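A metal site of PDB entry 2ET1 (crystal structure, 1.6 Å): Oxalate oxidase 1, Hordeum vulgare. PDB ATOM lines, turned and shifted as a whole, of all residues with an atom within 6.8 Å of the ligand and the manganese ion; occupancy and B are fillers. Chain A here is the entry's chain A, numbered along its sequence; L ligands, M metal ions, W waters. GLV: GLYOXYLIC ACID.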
ATOM      1  N   VAL A  56     -18.455  25.115   1.176  1.00  0.00           N
ATOM      2  CA  VAL A  56     -19.250  26.348   1.150  1.00  0.00           C
ATOM      3  C   VAL A  56     -18.520  27.401   0.311  1.00  0.00           C
ATOM      4  O   VAL A  56     -17.362  27.736   0.601  1.00  0.00           O
ATOM      5  CB  VAL A  56     -19.484  26.921   2.589  1.00  0.00           C
ATOM      6  CG1 VAL A  56     -20.364  28.188   2.541  1.00  0.00           C
ATOM      7  CG2 VAL A  56     -20.092  25.863   3.511  1.00  0.00           C
ATOM      8  N   THR A  57     -19.192  27.895  -0.737  1.00  0.00           N
ATOM      9  CA  THR A  57     -18.684  28.987  -1.555  1.00  0.00           C
ATOM     10  C   THR A  57     -19.492  30.240  -1.175  1.00  0.00           C
ATOM     11  O   THR A  57     -20.695  30.306  -1.420  1.00  0.00           O
ATOM     12  CB  THR A  57     -18.806  28.696  -3.072  1.00  0.00           C
ATOM     13  OG1 THR A  57     -18.114  27.479  -3.409  1.00  0.00           O
ATOM     14  CG2 THR A  57     -18.204  29.819  -3.904  1.00  0.00           C
ATOM     15  N   GLU A  58     -18.814  31.215  -0.573  1.00  0.00           N
ATOM     16  CA  GLU A  58     -19.514  32.380  -0.028  1.00  0.00           C
ATOM     17  C   GLU A  58     -19.664  33.532  -0.998  1.00  0.00           C
ATOM     18  O   GLU A  58     -18.754  33.840  -1.770  1.00  0.00           O
ATOM     19  CB  GLU A  58     -18.806  32.877   1.232  1.00  0.00           C
ATOM     20  CG  GLU A  58     -18.903  31.942   2.425  1.00  0.00           C
ATOM     21  CD  GLU A  58     -18.285  32.517   3.676  1.00  0.00           C
ATOM     22  OE1 GLU A  58     -19.053  32.862   4.604  1.00  0.00           O
ATOM     23  OE2 GLU A  58     -17.055  32.633   3.742  1.00  0.00           O
ATOM     24  N   ASN A  75     -24.975  32.102  -0.479  1.00  0.00           N
ATOM     25  CA  ASN A  75     -23.880  31.101  -0.559  1.00  0.00           C
ATOM     26  C   ASN A  75     -24.335  29.908  -1.401  1.00  0.00           C
ATOM     27  O   ASN A  75     -25.526  29.663  -1.531  1.00  0.00           O
ATOM     28  CB  ASN A  75     -23.502  30.543   0.829  1.00  0.00           C
ATOM     29  CG  ASN A  75     -22.978  31.595   1.812  1.00  0.00           C
ATOM     30  OD1 ASN A  75     -22.983  31.355   3.024  1.00  0.00           O
ATOM     31  ND2 ASN A  75     -22.514  32.726   1.304  1.00  0.00           N
ATOM     32  N   ARG A  76     -23.369  29.165  -1.951  1.00  0.00           N
ATOM     33  CA  ARG A  76     -23.606  27.860  -2.584  1.00  0.00           C
ATOM     34  C   ARG A  76     -22.974  26.786  -1.689  1.00  0.00           C
ATOM     35  O   ARG A  76     -21.906  27.019  -1.113  1.00  0.00           O
ATOM     36  CB  ARG A  76     -22.992  27.833  -3.987  1.00  0.00           C
ATOM     37  CG  ARG A  76     -22.987  26.459  -4.650  1.00  0.00           C
ATOM     38  CD  ARG A  76     -22.393  26.500  -6.069  1.00  0.00           C
ATOM     39  NE  ARG A  76     -22.318  25.138  -6.603  1.00  0.00           N
ATOM     40  CZ  ARG A  76     -22.502  24.804  -7.887  1.00  0.00           C
ATOM     41  NH1 ARG A  76     -22.757  25.736  -8.798  1.00  0.00           N
ATOM     42  NH2 ARG A  76     -22.422  23.534  -8.240  1.00  0.00           N
ATOM     43  N   VAL A  77     -23.622  25.622  -1.553  1.00  0.00           N
ATOM     44  CA  VAL A  77     -23.012  24.502  -0.788  1.00  0.00           C
ATOM     45  C   VAL A  77     -23.088  23.227  -1.622  1.00  0.00           C
ATOM     46  O   VAL A  77     -24.169  22.872  -2.093  1.00  0.00           O
ATOM     47  CB  VAL A  77     -23.672  24.288   0.606  1.00  0.00           C
ATOM     48  CG1 VAL A  77     -22.870  23.277   1.440  1.00  0.00           C
ATOM     49  CG2 VAL A  77     -23.784  25.617   1.352  1.00  0.00           C
ATOM     50  N   PHE A  79     -22.101  18.964  -1.890  1.00  0.00           N
ATOM     51  CA  PHE A  79     -21.995  17.796  -0.997  1.00  0.00           C
ATOM     52  C   PHE A  79     -21.552  16.519  -1.749  1.00  0.00           C
ATOM     53  O   PHE A  79     -22.208  16.124  -2.701  1.00  0.00           O
ATOM     54  CB  PHE A  79     -23.344  17.438  -0.342  1.00  0.00           C
ATOM     55  CG  PHE A  79     -23.970  18.538   0.496  1.00  0.00           C
ATOM     56  CD1 PHE A  79     -23.970  18.443   1.892  1.00  0.00           C
ATOM     57  CD2 PHE A  79     -24.633  19.611  -0.103  1.00  0.00           C
ATOM     58  CE1 PHE A  79     -24.574  19.431   2.676  1.00  0.00           C
ATOM     59  CE2 PHE A  79     -25.235  20.615   0.665  1.00  0.00           C
ATOM     60  CZ  PHE A  79     -25.219  20.512   2.072  1.00  0.00           C
ATOM     61  N   ASN A  85     -23.122  19.268   5.950  1.00  0.00           N
ATOM     62  CA  ASN A  85     -22.881  20.631   6.412  1.00  0.00           C
ATOM     63  C   ASN A  85     -23.323  20.598   7.879  1.00  0.00           C
ATOM     64  O   ASN A  85     -24.527  20.542   8.172  1.00  0.00           O
ATOM     65  CB  ASN A  85     -23.699  21.620   5.568  1.00  0.00           C
ATOM     66  CG  ASN A  85     -23.254  23.071   5.736  1.00  0.00           C
ATOM     67  OD1 ASN A  85     -22.131  23.352   6.160  1.00  0.00           O
ATOM     68  ND2 ASN A  85     -24.145  24.008   5.388  1.00  0.00           N
ATOM     69  N   HIS A  88     -24.846  24.100  12.658  1.00  0.00           N
ATOM     70  CA  HIS A  88     -24.303  25.455  12.697  1.00  0.00           C
ATOM     71  C   HIS A  88     -25.398  26.500  12.947  1.00  0.00           C
ATOM     72  O   HIS A  88     -26.588  26.163  12.895  1.00  0.00           O
ATOM     73  CB  HIS A  88     -23.499  25.780  11.403  1.00  0.00           C
ATOM     74  CG  HIS A  88     -24.319  25.841  10.133  1.00  0.00           C
ATOM     75  ND1 HIS A  88     -24.744  24.703   9.469  1.00  0.00           N
ATOM     76  CD2 HIS A  88     -24.752  26.896   9.394  1.00  0.00           C
ATOM     77  CE1 HIS A  88     -25.434  25.060   8.383  1.00  0.00           C
ATOM     78  NE2 HIS A  88     -25.431  26.378   8.318  1.00  0.00           N
ATOM     79  N   ILE A  89     -24.984  27.745  13.186  1.00  0.00           N
ATOM     80  CA  ILE A  89     -25.848  28.899  13.527  1.00  0.00           C
ATOM     81  C   ILE A  89     -25.387  30.132  12.759  1.00  0.00           C
ATOM     82  O   ILE A  89     -24.188  30.330  12.551  1.00  0.00           O
ATOM     83  CB  ILE A  89     -25.805  29.165  15.040  1.00  0.00           C
ATOM     84  CG1 ILE A  89     -26.532  28.015  15.762  1.00  0.00           C
ATOM     85  CG2 ILE A  89     -26.393  30.547  15.402  1.00  0.00           C
ATOM     86  CD1 ILE A  89     -26.542  28.068  17.236  1.00  0.00           C
ATOM     87  N   HIS A  90     -26.345  30.959  12.310  1.00  0.00           N
ATOM     88  CA  HIS A  90     -26.038  32.293  11.769  1.00  0.00           C
ATOM     89  C   HIS A  90     -26.475  33.331  12.790  1.00  0.00           C
ATOM     90  O   HIS A  90     -27.675  33.507  13.037  1.00  0.00           O
ATOM     91  CB  HIS A  90     -26.769  32.499  10.428  1.00  0.00           C
ATOM     92  CG  HIS A  90     -26.459  31.424   9.421  1.00  0.00           C
ATOM     93  ND1 HIS A  90     -25.203  31.290   8.870  1.00  0.00           N
ATOM     94  CD2 HIS A  90     -27.201  30.405   8.936  1.00  0.00           C
ATOM     95  CE1 HIS A  90     -25.188  30.221   8.075  1.00  0.00           C
ATOM     96  NE2 HIS A  90     -26.395  29.670   8.093  1.00  0.00           N
ATOM     97  N   GLU A  95     -32.150  32.467   7.057  1.00  0.00           N
ATOM     98  CA  GLU A  95     -31.730  31.838   5.793  1.00  0.00           C
ATOM     99  C   GLU A  95     -32.945  31.271   5.039  1.00  0.00           C
ATOM    100  O   GLU A  95     -33.881  30.732   5.667  1.00  0.00           O
ATOM    101  CB  GLU A  95     -30.754  30.699   6.102  1.00  0.00           C
ATOM    102  CG  GLU A  95     -30.282  29.869   4.893  1.00  0.00           C
ATOM    103  CD  GLU A  95     -29.344  28.744   5.295  1.00  0.00           C
ATOM    104  OE1 GLU A  95     -28.619  28.892   6.294  1.00  0.00           O
ATOM    105  OE2 GLU A  95     -29.351  27.679   4.605  1.00  0.00           O
ATOM    106  N   PHE A 129     -36.555  25.496   1.889  1.00  0.00           N
ATOM    107  CA  PHE A 129     -36.594  25.453   3.354  1.00  0.00           C
ATOM    108  C   PHE A 129     -36.261  26.822   3.941  1.00  0.00           C
ATOM    109  O   PHE A 129     -35.664  27.673   3.267  1.00  0.00           O
ATOM    110  CB  PHE A 129     -35.632  24.375   3.900  1.00  0.00           C
ATOM    111  CG  PHE A 129     -34.172  24.598   3.528  1.00  0.00           C
ATOM    112  CD1 PHE A 129     -33.334  25.423   4.312  1.00  0.00           C
ATOM    113  CD2 PHE A 129     -33.628  23.965   2.406  1.00  0.00           C
ATOM    114  CE1 PHE A 129     -31.996  25.604   3.961  1.00  0.00           C
ATOM    115  CE2 PHE A 129     -32.277  24.144   2.060  1.00  0.00           C
ATOM    116  CZ  PHE A 129     -31.462  24.989   2.832  1.00  0.00           C
ATOM    117  N   ILE A 131     -34.700  28.779   7.607  1.00  0.00           N
ATOM    118  CA  ILE A 131     -34.053  28.654   8.924  1.00  0.00           C
ATOM    119  C   ILE A 131     -34.181  29.983   9.695  1.00  0.00           C
ATOM    120  O   ILE A 131     -33.494  30.951   9.377  1.00  0.00           O
ATOM    121  CB  ILE A 131     -32.518  28.362   8.812  1.00  0.00           C
ATOM    122  CG1 ILE A 131     -32.151  27.388   7.656  1.00  0.00           C
ATOM    123  CG2 ILE A 131     -31.951  27.943  10.166  1.00  0.00           C
ATOM    124  CD1 ILE A 131     -32.539  25.926   7.854  1.00  0.00           C
ATOM    125  N   HIS A 137     -28.961  24.298  12.890  1.00  0.00           N
ATOM    126  CA  HIS A 137     -29.486  23.523  11.728  1.00  0.00           C
ATOM    127  C   HIS A 137     -28.351  22.784  11.006  1.00  0.00           C
ATOM    128  O   HIS A 137     -27.166  23.094  11.227  1.00  0.00           O
ATOM    129  CB  HIS A 137     -30.255  24.458  10.762  1.00  0.00           C
ATOM    130  CG  HIS A 137     -29.421  25.574  10.195  1.00  0.00           C
ATOM    131  ND1 HIS A 137     -28.967  26.623  10.968  1.00  0.00           N
ATOM    132  CD2 HIS A 137     -29.000  25.825   8.933  1.00  0.00           C
ATOM    133  CE1 HIS A 137     -28.287  27.463  10.205  1.00  0.00           C
ATOM    134  NE2 HIS A 137     -28.300  27.008   8.960  1.00  0.00           N
ATOM    135  N   GLN A 139     -27.405  19.949   7.267  1.00  0.00           N
ATOM    136  CA  GLN A 139     -27.814  19.192   6.066  1.00  0.00           C
ATOM    137  C   GLN A 139     -26.930  17.960   5.908  1.00  0.00           C
ATOM    138  O   GLN A 139     -25.758  17.971   6.298  1.00  0.00           O
ATOM    139  CB  GLN A 139     -27.757  20.035   4.772  1.00  0.00           C
ATOM    140  CG  GLN A 139     -28.689  21.258   4.760  1.00  0.00           C
ATOM    141  CD  GLN A 139     -28.031  22.508   5.340  1.00  0.00           C
ATOM    142  OE1 GLN A 139     -26.793  22.619   5.383  1.00  0.00           O
ATOM    143  NE2 GLN A 139     -28.854  23.464   5.744  1.00  0.00           N
ATOM    144  N   MET A 149     -27.008  23.025  -3.167  1.00  0.00           N
ATOM    145  CA  MET A 149     -28.069  23.975  -2.844  1.00  0.00           C
ATOM    146  C   MET A 149     -27.509  25.400  -2.944  1.00  0.00           C
ATOM    147  O   MET A 149     -26.287  25.620  -2.869  1.00  0.00           O
ATOM    148  CB  MET A 149     -28.613  23.733  -1.429  1.00  0.00           C
ATOM    149  CG  MET A 149     -27.599  23.914  -0.324  1.00  0.00           C
ATOM    150  SD  MET A 149     -28.290  23.555   1.296  1.00  0.00           S
ATOM    151  CE  MET A 149     -27.092  24.303   2.351  1.00  0.00           C
ATOM    152  N   VAL A 151     -28.413  29.203  -1.098  1.00  0.00           N
ATOM    153  CA  VAL A 151     -29.152  29.778   0.032  1.00  0.00           C
ATOM    154  C   VAL A 151     -28.934  31.290   0.097  1.00  0.00           C
ATOM    155  O   VAL A 151     -27.859  31.760  -0.250  1.00  0.00           O
ATOM    156  CB  VAL A 151     -28.759  29.112   1.388  1.00  0.00           C
ATOM    157  CG1 VAL A 151     -29.005  27.612   1.320  1.00  0.00           C
ATOM    158  CG2 VAL A 151     -27.304  29.355   1.739  1.00  0.00           C
ATOM    159  N   PHE A 153     -29.678  35.091   2.431  1.00  0.00           N
ATOM    160  CA  PHE A 153     -29.783  35.588   3.813  1.00  0.00           C
ATOM    161  C   PHE A 153     -30.299  37.027   3.831  1.00  0.00           C
ATOM    162  O   PHE A 153     -30.000  37.789   2.906  1.00  0.00           O
ATOM    163  CB  PHE A 153     -28.403  35.589   4.508  1.00  0.00           C
ATOM    164  CG  PHE A 153     -27.713  34.252   4.520  1.00  0.00           C
ATOM    165  CD1 PHE A 153     -26.821  33.906   3.502  1.00  0.00           C
ATOM    166  CD2 PHE A 153     -27.934  33.344   5.563  1.00  0.00           C
ATOM    167  CE1 PHE A 153     -26.189  32.652   3.506  1.00  0.00           C
ATOM    168  CE2 PHE A 153     -27.316  32.076   5.578  1.00  0.00           C
ATOM    169  CZ  PHE A 153     -26.422  31.739   4.537  1.00  0.00           C
ATOM    170  N   PRO A 158     -23.971  37.323   7.409  1.00  0.00           N
ATOM    171  CA  PRO A 158     -24.736  36.597   8.442  1.00  0.00           C
ATOM    172  C   PRO A 158     -23.879  36.018   9.567  1.00  0.00           C
ATOM    173  O   PRO A 158     -24.382  35.872  10.707  1.00  0.00           O
ATOM    174  CB  PRO A 158     -25.412  35.457   7.648  1.00  0.00           C
ATOM    175  CG  PRO A 158     -24.620  35.287   6.420  1.00  0.00           C
ATOM    176  CD  PRO A 158     -24.094  36.686   6.084  1.00  0.00           C
ATOM    177  N   GLY A 159     -22.624  35.675   9.256  1.00  0.00           N
ATOM    178  CA  GLY A 159     -21.723  34.970  10.200  1.00  0.00           C
ATOM    179  C   GLY A 159     -22.004  33.478  10.189  1.00  0.00           C
ATOM    180  O   GLY A 159     -23.115  33.055   9.896  1.00  0.00           O
ATOM    181  N   ILE A 160     -20.985  32.670  10.459  1.00  0.00           N
ATOM    182  CA  ILE A 160     -21.200  31.211  10.599  1.00  0.00           C
ATOM    183  C   ILE A 160     -20.538  30.710  11.881  1.00  0.00           C
ATOM    184  O   ILE A 160     -19.319  30.828  12.044  1.00  0.00           O
ATOM    185  CB  ILE A 160     -20.661  30.401   9.382  1.00  0.00           C
ATOM    186  CG1 ILE A 160     -21.189  30.951   8.047  1.00  0.00           C
ATOM    187  CG2 ILE A 160     -21.057  28.913   9.546  1.00  0.00           C
ATOM    188  CD1 ILE A 160     -20.482  30.348   6.824  1.00  0.00           C
ATOM    189  N   PHE A 162     -19.894  27.316  13.351  1.00  0.00           N
ATOM    190  CA  PHE A 162     -19.898  25.856  13.159  1.00  0.00           C
ATOM    191  C   PHE A 162     -19.784  25.212  14.541  1.00  0.00           C
ATOM    192  O   PHE A 162     -18.797  25.418  15.244  1.00  0.00           O
ATOM    193  CB  PHE A 162     -18.726  25.394  12.280  1.00  0.00           C
ATOM    194  CG  PHE A 162     -18.915  25.634  10.804  1.00  0.00           C
ATOM    195  CD1 PHE A 162     -18.120  26.566  10.127  1.00  0.00           C
ATOM    196  CD2 PHE A 162     -19.875  24.919  10.074  1.00  0.00           C
ATOM    197  CE1 PHE A 162     -18.260  26.771   8.752  1.00  0.00           C
ATOM    198  CE2 PHE A 162     -20.032  25.132   8.687  1.00  0.00           C
ATOM    199  CZ  PHE A 162     -19.221  26.064   8.029  1.00  0.00           C
HETATM  200  C1  GLV L   1     -23.833  28.186   3.950  1.00  0.00           C
HETATM  201  O1  GLV L   1     -23.399  29.381   4.616  1.00  0.00           O
HETATM  202  C2  GLV L   1     -24.961  27.582   4.737  1.00  0.00           C
HETATM  203  O2  GLV L   1     -25.352  26.415   4.451  1.00  0.00           O
HETATM  204  O3  GLV L   1     -25.472  28.277   5.631  1.00  0.00           O
HETATM  205 MN    MN M   1     -27.014  27.737   7.177  1.00  0.00          MN
HETATM  206  O   HOH W   1     -27.614  26.070   5.769  1.00  0.00           O
HETATM  207  O   HOH W   2     -23.487  32.082   5.860  1.00  0.00           O
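An oxygen (O1) of the ligand lies close to the side-chain amide oxygen (OD1) of Asn 75, at 2.6 Å. The side-chain amide nitrogen (ND2) of Asn 85 is in hydrogen-bond range of an oxygen (O2) of the ligand, at 2.9 Å.
The backbone carbonyl oxygen (O) of Glu 95 lies within hydrogen-bond range of the backbone NH (N) of Ile 131 (2.9 Å). O of Gly 159 is in hydrogen-bond range of ND1 of His 90, at 2.9 Å. N of Asn 75 sits at hydrogen-bond distance from O of Val 151 (2.9 Å). The backbone NH of Asn 85 is in hydrogen-bond range of the backbone carbonyl oxygen of Gln 139 (3.0 Å). O of Met 149 lies within hydrogen-bond range of N of Val 77 (3.0 Å).
Val 56 touches the ligand (CG1 to C1, 3.7 Å). Val 77 touches the ligand. Met 149 touches the ligand. Phe 153 touches the ligand. CD1 of Ile 160 touches O1 of the ligand, 3.8 Å away. Ten residues have an atom within 4 Å of the ligand: Val 56, Asn 75, Val 77, Asn 85, His 88, His 90, Glu 95, Met 149, Phe 153 and Ile 160. The nearest printed residue that does not touch the ligand is Gln 139 (4.2 Å).
The nearest printed residue that does not touch the manganese ion is Phe 153 (4.6 Å).
The side-chain carboxylate (OE1) of Glu 95 binds the manganese ion. The manganese ion is bound by NE2 of His 90 (2.2 Å). The manganese ion is bound by O3 of the ligand (2.2 Å). The manganese ion is bound by water W1. NE2 of His 137 is bound to the manganese ion (2.3 Å). The manganese ion is bound by NE2 of His 88.
Water W1 lies within hydrogen-bond range of the side-chain carboxylate of Glu 95, an oxygen (O2) of the ligand and the side-chain amide nitrogen of Gln 139. Water W2 lies within hydrogen-bond range of the side-chain amide oxygen of Asn 75 (3.0 Å) and an oxygen (O1) of the ligand (3.0 Å).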
